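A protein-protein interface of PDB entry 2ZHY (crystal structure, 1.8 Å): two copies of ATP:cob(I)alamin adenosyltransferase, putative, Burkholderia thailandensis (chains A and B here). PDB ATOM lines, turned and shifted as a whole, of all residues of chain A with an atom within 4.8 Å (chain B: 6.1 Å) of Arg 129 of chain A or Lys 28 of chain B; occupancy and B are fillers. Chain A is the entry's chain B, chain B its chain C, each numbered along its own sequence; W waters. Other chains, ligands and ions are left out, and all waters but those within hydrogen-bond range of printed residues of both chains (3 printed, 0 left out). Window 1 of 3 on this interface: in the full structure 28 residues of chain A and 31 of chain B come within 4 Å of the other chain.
Thr 126 of chain A touches Asp 40 of chain B (CG2 to CG, 3.6 Å).
Arg 129 of chain A touches Lys 28 of chain B.
Lys 28 of chain B touches Arg 133 of chain A.
Arg 133 of chain A touches Asp 29 of chain B.
Ile 33 of chain B touches Arg 133 of chain A.
NE of Arg 133 of chain A touches CA of Ala 34 of chain B (3.5 Å).
NH1 of Arg 133 of chain A touches CA of Gly 37 of chain B, at 3.8 Å.
Gly 16 of chain B touches Val 136 of chain A (O to CG1, 3.95 Å).
Val 136 of chain A touches Arg 27 of chain B.
Asn 153 of chain A touches Gly 13 of chain B.
Water W2 lies within hydrogen-bond range of O of Gly 13 of chain B (2.7 Å), OE2 of Glu 132 of chain A (2.8 Å), N of Gly 16 of chain B (3.3 Å) and NZ of Lys 28 of chain B (3.4 Å).
Water W1 lies within hydrogen-bond range of the backbone carbonyl oxygen (O) of Thr 126 of chain A (2.8 Å), the guanidinium group (NH1) of Arg 133 of chain A (3.0 Å) and the backbone carbonyl oxygen (O) of Gly 37 of chain B (3.1 Å).
Water W3 lies within hydrogen-bond range of NH2 of Arg 133 of chain A (2.8 Å) and O of Gly 37 of chain B (3.3 Å).
Of the printed residues of chain B, Thr 126 of chain A touches Asp 40 (3.6 Å).
Of chain B, only Lys 28 (3.7 Å) comes within 4 Å of Arg 129 of chain A.
Arg 130 of chain A touches none of the printed residues of chain B.
Of the printed residues of chain A, Thr 12 of chain B touches Asn 153.
Thr 18 of chain B touches none of the printed residues of chain A.
Of the printed residues of chain A, Lys 28 of chain B touches Arg 129, Glu 132, Arg 133 and Asn 153.
Of the printed residues of chain A, Asp 40 of chain B touches Arg 125 and Thr 126.
The nearest residue of chain A that does not touch Lys 28 of chain B is Val 136 of chain A (4.1 Å).
The nearest printed residue of chain B that does not touch Thr 126 of chain A is Gly 37 of chain B (4.7 Å).
Of the 15 printed residues of chain B, 11 touch a printed residue of chain A.
Printed residues of chain A that touch a printed residue of chain B: Arg 125, Thr 126, Arg 129, Glu 132, Arg 133, Val 136 and Asn 153.
Hydrophobic or aromatic side chains of chain A that line the printed part of chain B: Val 136.
Among the printed residues, Asp or Glu carboxylates within 4 Å of a Lys or Arg side-chain nitrogen of the other chain: Arg 125 of chain A with Asp 40 of chain B (2.8 Å) and Glu 132 of chain A with Lys 28 of chain B (2.5 Å).
No position is printed for both chains.
Of the 15 pairs that touch across the chains among the printed residues, none has its exchanged pair printed and touching as well.
The guanidinium group of Arg 125 of chain A is in salt-bridge range of the side-chain carboxylate of Asp 40 of chain B (2.8 Å).
The side-chain amino group (NZ) of Lys 28 of chain B is in salt-bridge range of the side-chain carboxylate (OE2) of Glu 132 of chain A, at 2.5 Å.
O of Thr 12 of chain B lies close to OD1 of Asn 153 of chain A, 3.4 Å away.
OD1 of Asn 153 of chain A sits close to OD1 of Asp 14 of chain B (2.7 Å).
The side-chain amino group (NZ) of Lys 28 of chain B sits close to the side-chain amide nitrogen (ND2) of Asn 153 of chain A, 3.3 Å away.
The guanidinium group (NH1) of Arg 129 of chain A lies close to the side-chain amide nitrogen (ND2) of Asn 153 of chain A.
The guanidinium group (NE) of Arg 129 of chain A sits close to the side-chain hydroxyl (OG) of Ser 156 of chain A (3.4 Å).
OD1 of Asp 157 of chain A is in salt-bridge range of NH2 of Arg 129 of chain A.
The backbone carbonyl oxygen (O) of Gly 13 of chain B lies within hydrogen-bond range of the side-chain amino group (NZ) of Lys 28 of chain B.
The backbone NH of Lys 28 of chain B lies within hydrogen-bond range of the backbone carbonyl oxygen of Gly 16 of chain B (2.8 Å).
NE of Arg 27 of chain B lies within salt-bridge range of OD2 of Asp 29 of chain B (2.8 Å).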
ATOM      1  N   ARG A 125      20.846  20.636   3.722  1.00  0.00           N
ATOM      2  CA  ARG A 125      20.650  19.188   3.740  1.00  0.00           C
ATOM      3  C   ARG A 125      21.279  18.511   2.515  1.00  0.00           C
ATOM      4  O   ARG A 125      21.927  17.473   2.647  1.00  0.00           O
ATOM      5  CB  ARG A 125      19.150  18.856   3.793  1.00  0.00           C
ATOM      6  CG  ARG A 125      18.801  17.358   3.673  1.00  0.00           C
ATOM      7  CD  ARG A 125      17.285  17.146   3.594  1.00  0.00           C
ATOM      8  NE  ARG A 125      16.709  17.789   2.409  1.00  0.00           N
ATOM      9  CZ  ARG A 125      16.765  17.286   1.174  1.00  0.00           C
ATOM     10  NH1 ARG A 125      17.354  16.119   0.944  1.00  0.00           N
ATOM     11  NH2 ARG A 125      16.266  17.974   0.153  1.00  0.00           N
ATOM     12  N   THR A 126      21.087  19.087   1.327  1.00  0.00           N
ATOM     13  CA  THR A 126      21.643  18.484   0.118  1.00  0.00           C
ATOM     14  C   THR A 126      23.158  18.636   0.063  1.00  0.00           C
ATOM     15  O   THR A 126      23.859  17.735  -0.387  1.00  0.00           O
ATOM     16  CB  THR A 126      21.004  19.071  -1.181  1.00  0.00           C
ATOM     17  OG1 THR A 126      21.271  20.474  -1.271  1.00  0.00           O
ATOM     18  CG2 THR A 126      19.492  18.839  -1.179  1.00  0.00           C
ATOM     19  N   VAL A 127      23.670  19.769   0.525  1.00  0.00           N
ATOM     20  CA  VAL A 127      25.108  19.975   0.532  1.00  0.00           C
ATOM     21  C   VAL A 127      25.719  19.039   1.568  1.00  0.00           C
ATOM     22  O   VAL A 127      26.849  18.569   1.407  1.00  0.00           O
ATOM     23  CB  VAL A 127      25.469  21.431   0.874  1.00  0.00           C
ATOM     24  CG1 VAL A 127      26.987  21.593   0.914  1.00  0.00           C
ATOM     25  CG2 VAL A 127      24.872  22.371  -0.178  1.00  0.00           C
ATOM     26  N   CYS A 128      24.960  18.767   2.629  1.00  0.00           N
ATOM     27  CA  CYS A 128      25.425  17.863   3.675  1.00  0.00           C
ATOM     28  C   CYS A 128      25.558  16.467   3.072  1.00  0.00           C
ATOM     29  O   CYS A 128      26.547  15.776   3.301  1.00  0.00           O
ATOM     30  CB  CYS A 128      24.446  17.838   4.850  1.00  0.00           C
ATOM     31  SG  CYS A 128      25.039  16.857   6.274  1.00  0.00           S
ATOM     32  N   ARG A 129      24.557  16.059   2.292  1.00  0.00           N
ATOM     33  CA  ARG A 129      24.586  14.756   1.636  1.00  0.00           C
ATOM     34  C   ARG A 129      25.764  14.700   0.665  1.00  0.00           C
ATOM     35  O   ARG A 129      26.410  13.667   0.519  1.00  0.00           O
ATOM     36  CB  ARG A 129      23.276  14.509   0.881  1.00  0.00           C
ATOM     37  CG  ARG A 129      22.093  14.160   1.775  1.00  0.00           C
ATOM     38  CD  ARG A 129      22.352  12.863   2.522  1.00  0.00           C
ATOM     39  NE  ARG A 129      21.188  12.410   3.282  1.00  0.00           N
ATOM     40  CZ  ARG A 129      21.226  11.460   4.215  1.00  0.00           C
ATOM     41  NH1 ARG A 129      22.372  10.851   4.507  1.00  0.00           N
ATOM     42  NH2 ARG A 129      20.118  11.127   4.869  1.00  0.00           N
ATOM     43  N   ARG A 130      26.035  15.816  -0.003  1.00  0.00           N
ATOM     44  CA  ARG A 130      27.155  15.892  -0.932  1.00  0.00           C
ATOM     45  C   ARG A 130      28.472  15.682  -0.176  1.00  0.00           C
ATOM     46  O   ARG A 130      29.371  14.984  -0.647  1.00  0.00           O
ATOM     47  CB  ARG A 130      27.170  17.255  -1.631  1.00  0.00           C
ATOM     48  CG  ARG A 130      28.404  17.504  -2.476  1.00  0.00           C
ATOM     49  CD  ARG A 130      28.047  18.230  -3.775  1.00  0.00           C
ATOM     50  NE  ARG A 130      27.430  19.540  -3.559  1.00  0.00           N
ATOM     51  CZ  ARG A 130      28.080  20.631  -3.161  1.00  0.00           C
ATOM     52  NH1 ARG A 130      29.389  20.591  -2.918  1.00  0.00           N
ATOM     53  NH2 ARG A 130      27.426  21.779  -3.043  1.00  0.00           N
ATOM     54  N   ALA A 131      28.584  16.288   1.001  1.00  0.00           N
ATOM     55  CA  ALA A 131      29.797  16.146   1.802  1.00  0.00           C
ATOM     56  C   ALA A 131      29.921  14.692   2.255  1.00  0.00           C
ATOM     57  O   ALA A 131      31.023  14.149   2.341  1.00  0.00           O
ATOM     58  CB  ALA A 131      29.740  17.075   3.015  1.00  0.00           C
ATOM     59  N   GLU A 132      28.784  14.066   2.548  1.00  0.00           N
ATOM     60  CA  GLU A 132      28.795  12.673   2.981  1.00  0.00           C
ATOM     61  C   GLU A 132      29.328  11.776   1.867  1.00  0.00           C
ATOM     62  O   GLU A 132      30.068  10.834   2.135  1.00  0.00           O
ATOM     63  CB  GLU A 132      27.393  12.216   3.392  1.00  0.00           C
ATOM     64  CG  GLU A 132      27.305  10.714   3.704  1.00  0.00           C
ATOM     65  CD  GLU A 132      25.938  10.296   4.228  1.00  0.00           C
ATOM     66  OE1 GLU A 132      24.925  10.842   3.746  1.00  0.00           O
ATOM     67  OE2 GLU A 132      25.878   9.415   5.116  1.00  0.00           O
ATOM     68  N   ARG A 133      28.948  12.064   0.622  1.00  0.00           N
ATOM     69  CA  ARG A 133      29.422  11.268  -0.510  1.00  0.00           C
ATOM     70  C   ARG A 133      30.942  11.398  -0.631  1.00  0.00           C
ATOM     71  O   ARG A 133      31.635  10.424  -0.931  1.00  0.00           O
ATOM     72  CB  ARG A 133      28.738  11.709  -1.820  1.00  0.00           C
ATOM     73  CG  ARG A 133      27.218  11.459  -1.859  1.00  0.00           C
ATOM     74  CD  ARG A 133      26.660  11.520  -3.288  1.00  0.00           C
ATOM     75  NE  ARG A 133      26.761  12.853  -3.888  1.00  0.00           N
ATOM     76  CZ  ARG A 133      25.946  13.871  -3.610  1.00  0.00           C
ATOM     77  NH1 ARG A 133      24.958  13.726  -2.737  1.00  0.00           N
ATOM     78  NH2 ARG A 133      26.117  15.034  -4.219  1.00  0.00           N
ATOM     79  N   VAL A 136      32.669   9.509   2.219  1.00  0.00           N
ATOM     80  CA  VAL A 136      32.582   8.082   1.915  1.00  0.00           C
ATOM     81  C   VAL A 136      33.610   7.692   0.857  1.00  0.00           C
ATOM     82  O   VAL A 136      34.265   6.664   0.982  1.00  0.00           O
ATOM     83  CB  VAL A 136      31.166   7.703   1.422  1.00  0.00           C
ATOM     84  CG1 VAL A 136      31.166   6.294   0.835  1.00  0.00           C
ATOM     85  CG2 VAL A 136      30.183   7.782   2.580  1.00  0.00           C
ATOM     86  N   ASN A 153      25.687  11.910   8.329  1.00  0.00           N
ATOM     87  CA  ASN A 153      24.549  11.064   7.997  1.00  0.00           C
ATOM     88  C   ASN A 153      23.358  11.534   8.838  1.00  0.00           C
ATOM     89  O   ASN A 153      22.250  11.701   8.328  1.00  0.00           O
ATOM     90  CB  ASN A 153      24.856   9.597   8.317  1.00  0.00           C
ATOM     91  CG  ASN A 153      23.673   8.680   8.052  1.00  0.00           C
ATOM     92  OD1 ASN A 153      23.484   7.672   8.743  1.00  0.00           O
ATOM     93  ND2 ASN A 153      22.875   9.016   7.042  1.00  0.00           N
ATOM     94  N   SER A 156      22.202  15.328   8.013  1.00  0.00           N
ATOM     95  CA  SER A 156      21.349  15.435   6.832  1.00  0.00           C
ATOM     96  C   SER A 156      19.893  15.294   7.274  1.00  0.00           C
ATOM     97  O   SER A 156      19.042  16.094   6.904  1.00  0.00           O
ATOM     98  CB  SER A 156      21.678  14.335   5.813  1.00  0.00           C
ATOM     99  OG  SER A 156      22.987  14.486   5.294  1.00  0.00           O
ATOM    100  N   ASP A 157      19.610  14.269   8.072  1.00  0.00           N
ATOM    101  CA  ASP A 157      18.250  14.047   8.554  1.00  0.00           C
ATOM    102  C   ASP A 157      17.769  15.158   9.480  1.00  0.00           C
ATOM    103  O   ASP A 157      16.582  15.491   9.489  1.00  0.00           O
ATOM    104  CB  ASP A 157      18.149  12.703   9.280  1.00  0.00           C
ATOM    105  CG  ASP A 157      18.316  11.526   8.343  1.00  0.00           C
ATOM    106  OD1 ASP A 157      17.813  11.604   7.201  1.00  0.00           O
ATOM    107  OD2 ASP A 157      18.938  10.525   8.747  1.00  0.00           O
ATOM    108  N   THR B  12      20.251   3.658   9.795  1.00  0.00           N
ATOM    109  CA  THR B  12      20.363   3.227   8.410  1.00  0.00           C
ATOM    110  C   THR B  12      21.261   4.216   7.685  1.00  0.00           C
ATOM    111  O   THR B  12      21.139   5.427   7.875  1.00  0.00           O
ATOM    112  CB  THR B  12      18.993   3.188   7.708  1.00  0.00           C
ATOM    113  OG1 THR B  12      18.089   2.384   8.473  1.00  0.00           O
ATOM    114  CG2 THR B  12      19.134   2.588   6.316  1.00  0.00           C
ATOM    115  N   GLY B  13      22.177   3.693   6.877  1.00  0.00           N
ATOM    116  CA  GLY B  13      23.082   4.544   6.134  1.00  0.00           C
ATOM    117  C   GLY B  13      24.389   4.831   6.844  1.00  0.00           C
ATOM    118  O   GLY B  13      25.294   5.412   6.252  1.00  0.00           O
ATOM    119  N   ASP B  14      24.499   4.434   8.111  1.00  0.00           N
ATOM    120  CA  ASP B  14      25.727   4.678   8.859  1.00  0.00           C
ATOM    121  C   ASP B  14      26.935   3.993   8.227  1.00  0.00           C
ATOM    122  O   ASP B  14      28.061   4.468   8.367  1.00  0.00           O
ATOM    123  CB  ASP B  14      25.587   4.220  10.319  1.00  0.00           C
ATOM    124  CG  ASP B  14      25.028   5.309  11.234  1.00  0.00           C
ATOM    125  OD1 ASP B  14      24.868   6.463  10.781  1.00  0.00           O
ATOM    126  OD2 ASP B  14      24.758   5.010  12.418  1.00  0.00           O
ATOM    127  N   GLY B  16      27.790   3.936   5.228  1.00  0.00           N
ATOM    128  CA  GLY B  16      28.181   4.551   3.973  1.00  0.00           C
ATOM    129  C   GLY B  16      27.423   4.062   2.754  1.00  0.00           C
ATOM    130  O   GLY B  16      27.893   4.224   1.627  1.00  0.00           O
ATOM    131  N   THR B  17      26.262   3.451   2.968  1.00  0.00           N
ATOM    132  CA  THR B  17      25.447   2.979   1.854  1.00  0.00           C
ATOM    133  C   THR B  17      24.063   3.612   1.941  1.00  0.00           C
ATOM    134  O   THR B  17      23.693   4.194   2.963  1.00  0.00           O
ATOM    135  CB  THR B  17      25.275   1.434   1.853  1.00  0.00           C
ATOM    136  OG1 THR B  17      24.543   1.030   3.016  1.00  0.00           O
ATOM    137  CG2 THR B  17      26.629   0.742   1.842  1.00  0.00           C
ATOM    138  N   THR B  18      23.309   3.505   0.854  1.00  0.00           N
ATOM    139  CA  THR B  18      21.957   4.042   0.789  1.00  0.00           C
ATOM    140  C   THR B  18      21.132   3.103  -0.088  1.00  0.00           C
ATOM    141  O   THR B  18      21.676   2.429  -0.965  1.00  0.00           O
ATOM    142  CB  THR B  18      21.951   5.468   0.195  1.00  0.00           C
ATOM    143  OG1 THR B  18      20.601   5.940   0.101  1.00  0.00           O
ATOM    144  CG2 THR B  18      22.593   5.480  -1.178  1.00  0.00           C
ATOM    145  N   VAL B  26      23.604   0.521  -2.243  1.00  0.00           N
ATOM    146  CA  VAL B  26      24.787   1.008  -2.936  1.00  0.00           C
ATOM    147  C   VAL B  26      25.585   1.962  -2.054  1.00  0.00           C
ATOM    148  O   VAL B  26      25.019   2.639  -1.196  1.00  0.00           O
ATOM    149  CB  VAL B  26      24.399   1.744  -4.240  1.00  0.00           C
ATOM    150  CG1 VAL B  26      25.637   2.060  -5.042  1.00  0.00           C
ATOM    151  CG2 VAL B  26      23.443   0.893  -5.061  1.00  0.00           C
ATOM    152  N   ARG B  27      26.897   2.012  -2.265  1.00  0.00           N
ATOM    153  CA  ARG B  27      27.750   2.904  -1.491  1.00  0.00           C
ATOM    154  C   ARG B  27      27.422   4.331  -1.931  1.00  0.00           C
ATOM    155  O   ARG B  27      27.203   4.584  -3.115  1.00  0.00           O
ATOM    156  CB  ARG B  27      29.229   2.583  -1.733  1.00  0.00           C
ATOM    157  CG  ARG B  27      30.133   3.060  -0.611  1.00  0.00           C
ATOM    158  CD  ARG B  27      31.536   2.480  -0.725  1.00  0.00           C
ATOM    159  NE  ARG B  27      32.282   3.041  -1.847  1.00  0.00           N
ATOM    160  CZ  ARG B  27      33.495   2.640  -2.209  1.00  0.00           C
ATOM    161  NH1 ARG B  27      34.099   1.669  -1.537  1.00  0.00           N
ATOM    162  NH2 ARG B  27      34.110   3.212  -3.234  1.00  0.00           N
ATOM    163  N   LYS B  28      27.383   5.253  -0.974  1.00  0.00           N
ATOM    164  CA  LYS B  28      27.027   6.640  -1.245  1.00  0.00           C
ATOM    165  C   LYS B  28      27.843   7.415  -2.275  1.00  0.00           C
ATOM    166  O   LYS B  28      27.366   8.423  -2.797  1.00  0.00           O
ATOM    167  CB  LYS B  28      26.945   7.406   0.079  1.00  0.00           C
ATOM    168  CG  LYS B  28      25.722   6.981   0.890  1.00  0.00           C
ATOM    169  CD  LYS B  28      25.613   7.656   2.250  1.00  0.00           C
ATOM    170  CE  LYS B  28      24.309   7.231   2.930  1.00  0.00           C
ATOM    171  NZ  LYS B  28      24.226   7.628   4.355  1.00  0.00           N
ATOM    172  N   ASP B  29      29.055   6.962  -2.581  1.00  0.00           N
ATOM    173  CA  ASP B  29      29.868   7.650  -3.582  1.00  0.00           C
ATOM    174  C   ASP B  29      29.620   7.097  -4.994  1.00  0.00           C
ATOM    175  O   ASP B  29      30.317   7.465  -5.942  1.00  0.00           O
ATOM    176  CB  ASP B  29      31.360   7.545  -3.252  1.00  0.00           C
ATOM    177  CG  ASP B  29      31.844   6.112  -3.172  1.00  0.00           C
ATOM    178  OD1 ASP B  29      33.073   5.899  -3.235  1.00  0.00           O
ATOM    179  OD2 ASP B  29      31.006   5.199  -3.032  1.00  0.00           O
ATOM    180  N   ASP B  30      28.632   6.217  -5.132  1.00  0.00           N
ATOM    181  CA  ASP B  30      28.303   5.634  -6.434  1.00  0.00           C
ATOM    182  C   ASP B  30      27.755   6.703  -7.375  1.00  0.00           C
ATOM    183  O   ASP B  30      26.985   7.564  -6.959  1.00  0.00           O
ATOM    184  CB  ASP B  30      27.269   4.517  -6.266  1.00  0.00           C
ATOM    185  CG  ASP B  30      26.932   3.821  -7.578  1.00  0.00           C
ATOM    186  OD1 ASP B  30      26.155   4.379  -8.382  1.00  0.00           O
ATOM    187  OD2 ASP B  30      27.456   2.711  -7.807  1.00  0.00           O
ATOM    188  N   ILE B  33      24.157   7.607  -7.080  1.00  0.00           N
ATOM    189  CA  ILE B  33      23.812   8.369  -5.887  1.00  0.00           C
ATOM    190  C   ILE B  33      24.173   9.847  -6.038  1.00  0.00           C
ATOM    191  O   ILE B  33      23.444  10.710  -5.561  1.00  0.00           O
ATOM    192  CB  ILE B  33      24.506   7.781  -4.633  1.00  0.00           C
ATOM    193  CG1 ILE B  33      24.166   6.291  -4.512  1.00  0.00           C
ATOM    194  CG2 ILE B  33      24.050   8.526  -3.370  1.00  0.00           C
ATOM    195  CD1 ILE B  33      22.675   5.982  -4.644  1.00  0.00           C
ATOM    196  N   ALA B  34      25.294  10.135  -6.698  1.00  0.00           N
ATOM    197  CA  ALA B  34      25.720  11.517  -6.918  1.00  0.00           C
ATOM    198  C   ALA B  34      24.726  12.214  -7.849  1.00  0.00           C
ATOM    199  O   ALA B  34      24.408  13.385  -7.661  1.00  0.00           O
ATOM    200  CB  ALA B  34      27.126  11.550  -7.527  1.00  0.00           C
ATOM    201  N   GLY B  37      21.639  12.936  -5.839  1.00  0.00           N
ATOM    202  CA  GLY B  37      21.906  14.021  -4.906  1.00  0.00           C
ATOM    203  C   GLY B  37      21.947  15.389  -5.569  1.00  0.00           C
ATOM    204  O   GLY B  37      21.400  16.350  -5.028  1.00  0.00           O
ATOM    205  N   ASP B  40      18.541  16.576  -6.374  1.00  0.00           N
ATOM    206  CA  ASP B  40      17.915  16.996  -5.127  1.00  0.00           C
ATOM    207  C   ASP B  40      18.426  18.399  -4.756  1.00  0.00           C
ATOM    208  O   ASP B  40      17.644  19.261  -4.348  1.00  0.00           O
ATOM    209  CB  ASP B  40      18.258  15.992  -4.020  1.00  0.00           C
ATOM    210  CG  ASP B  40      17.520  16.267  -2.722  1.00  0.00           C
ATOM    211  OD1 ASP B  40      17.799  15.575  -1.720  1.00  0.00           O
ATOM    212  OD2 ASP B  40      16.663  17.172  -2.696  1.00  0.00           O
HETATM  213  O   HOH W   1      23.114  16.062  -2.453  1.00  0.00           O
HETATM  214  O   HOH W   2      27.328   7.150   5.786  1.00  0.00           O
HETATM  215  O   HOH W   3      24.508  17.274  -4.548  1.00  0.00           O
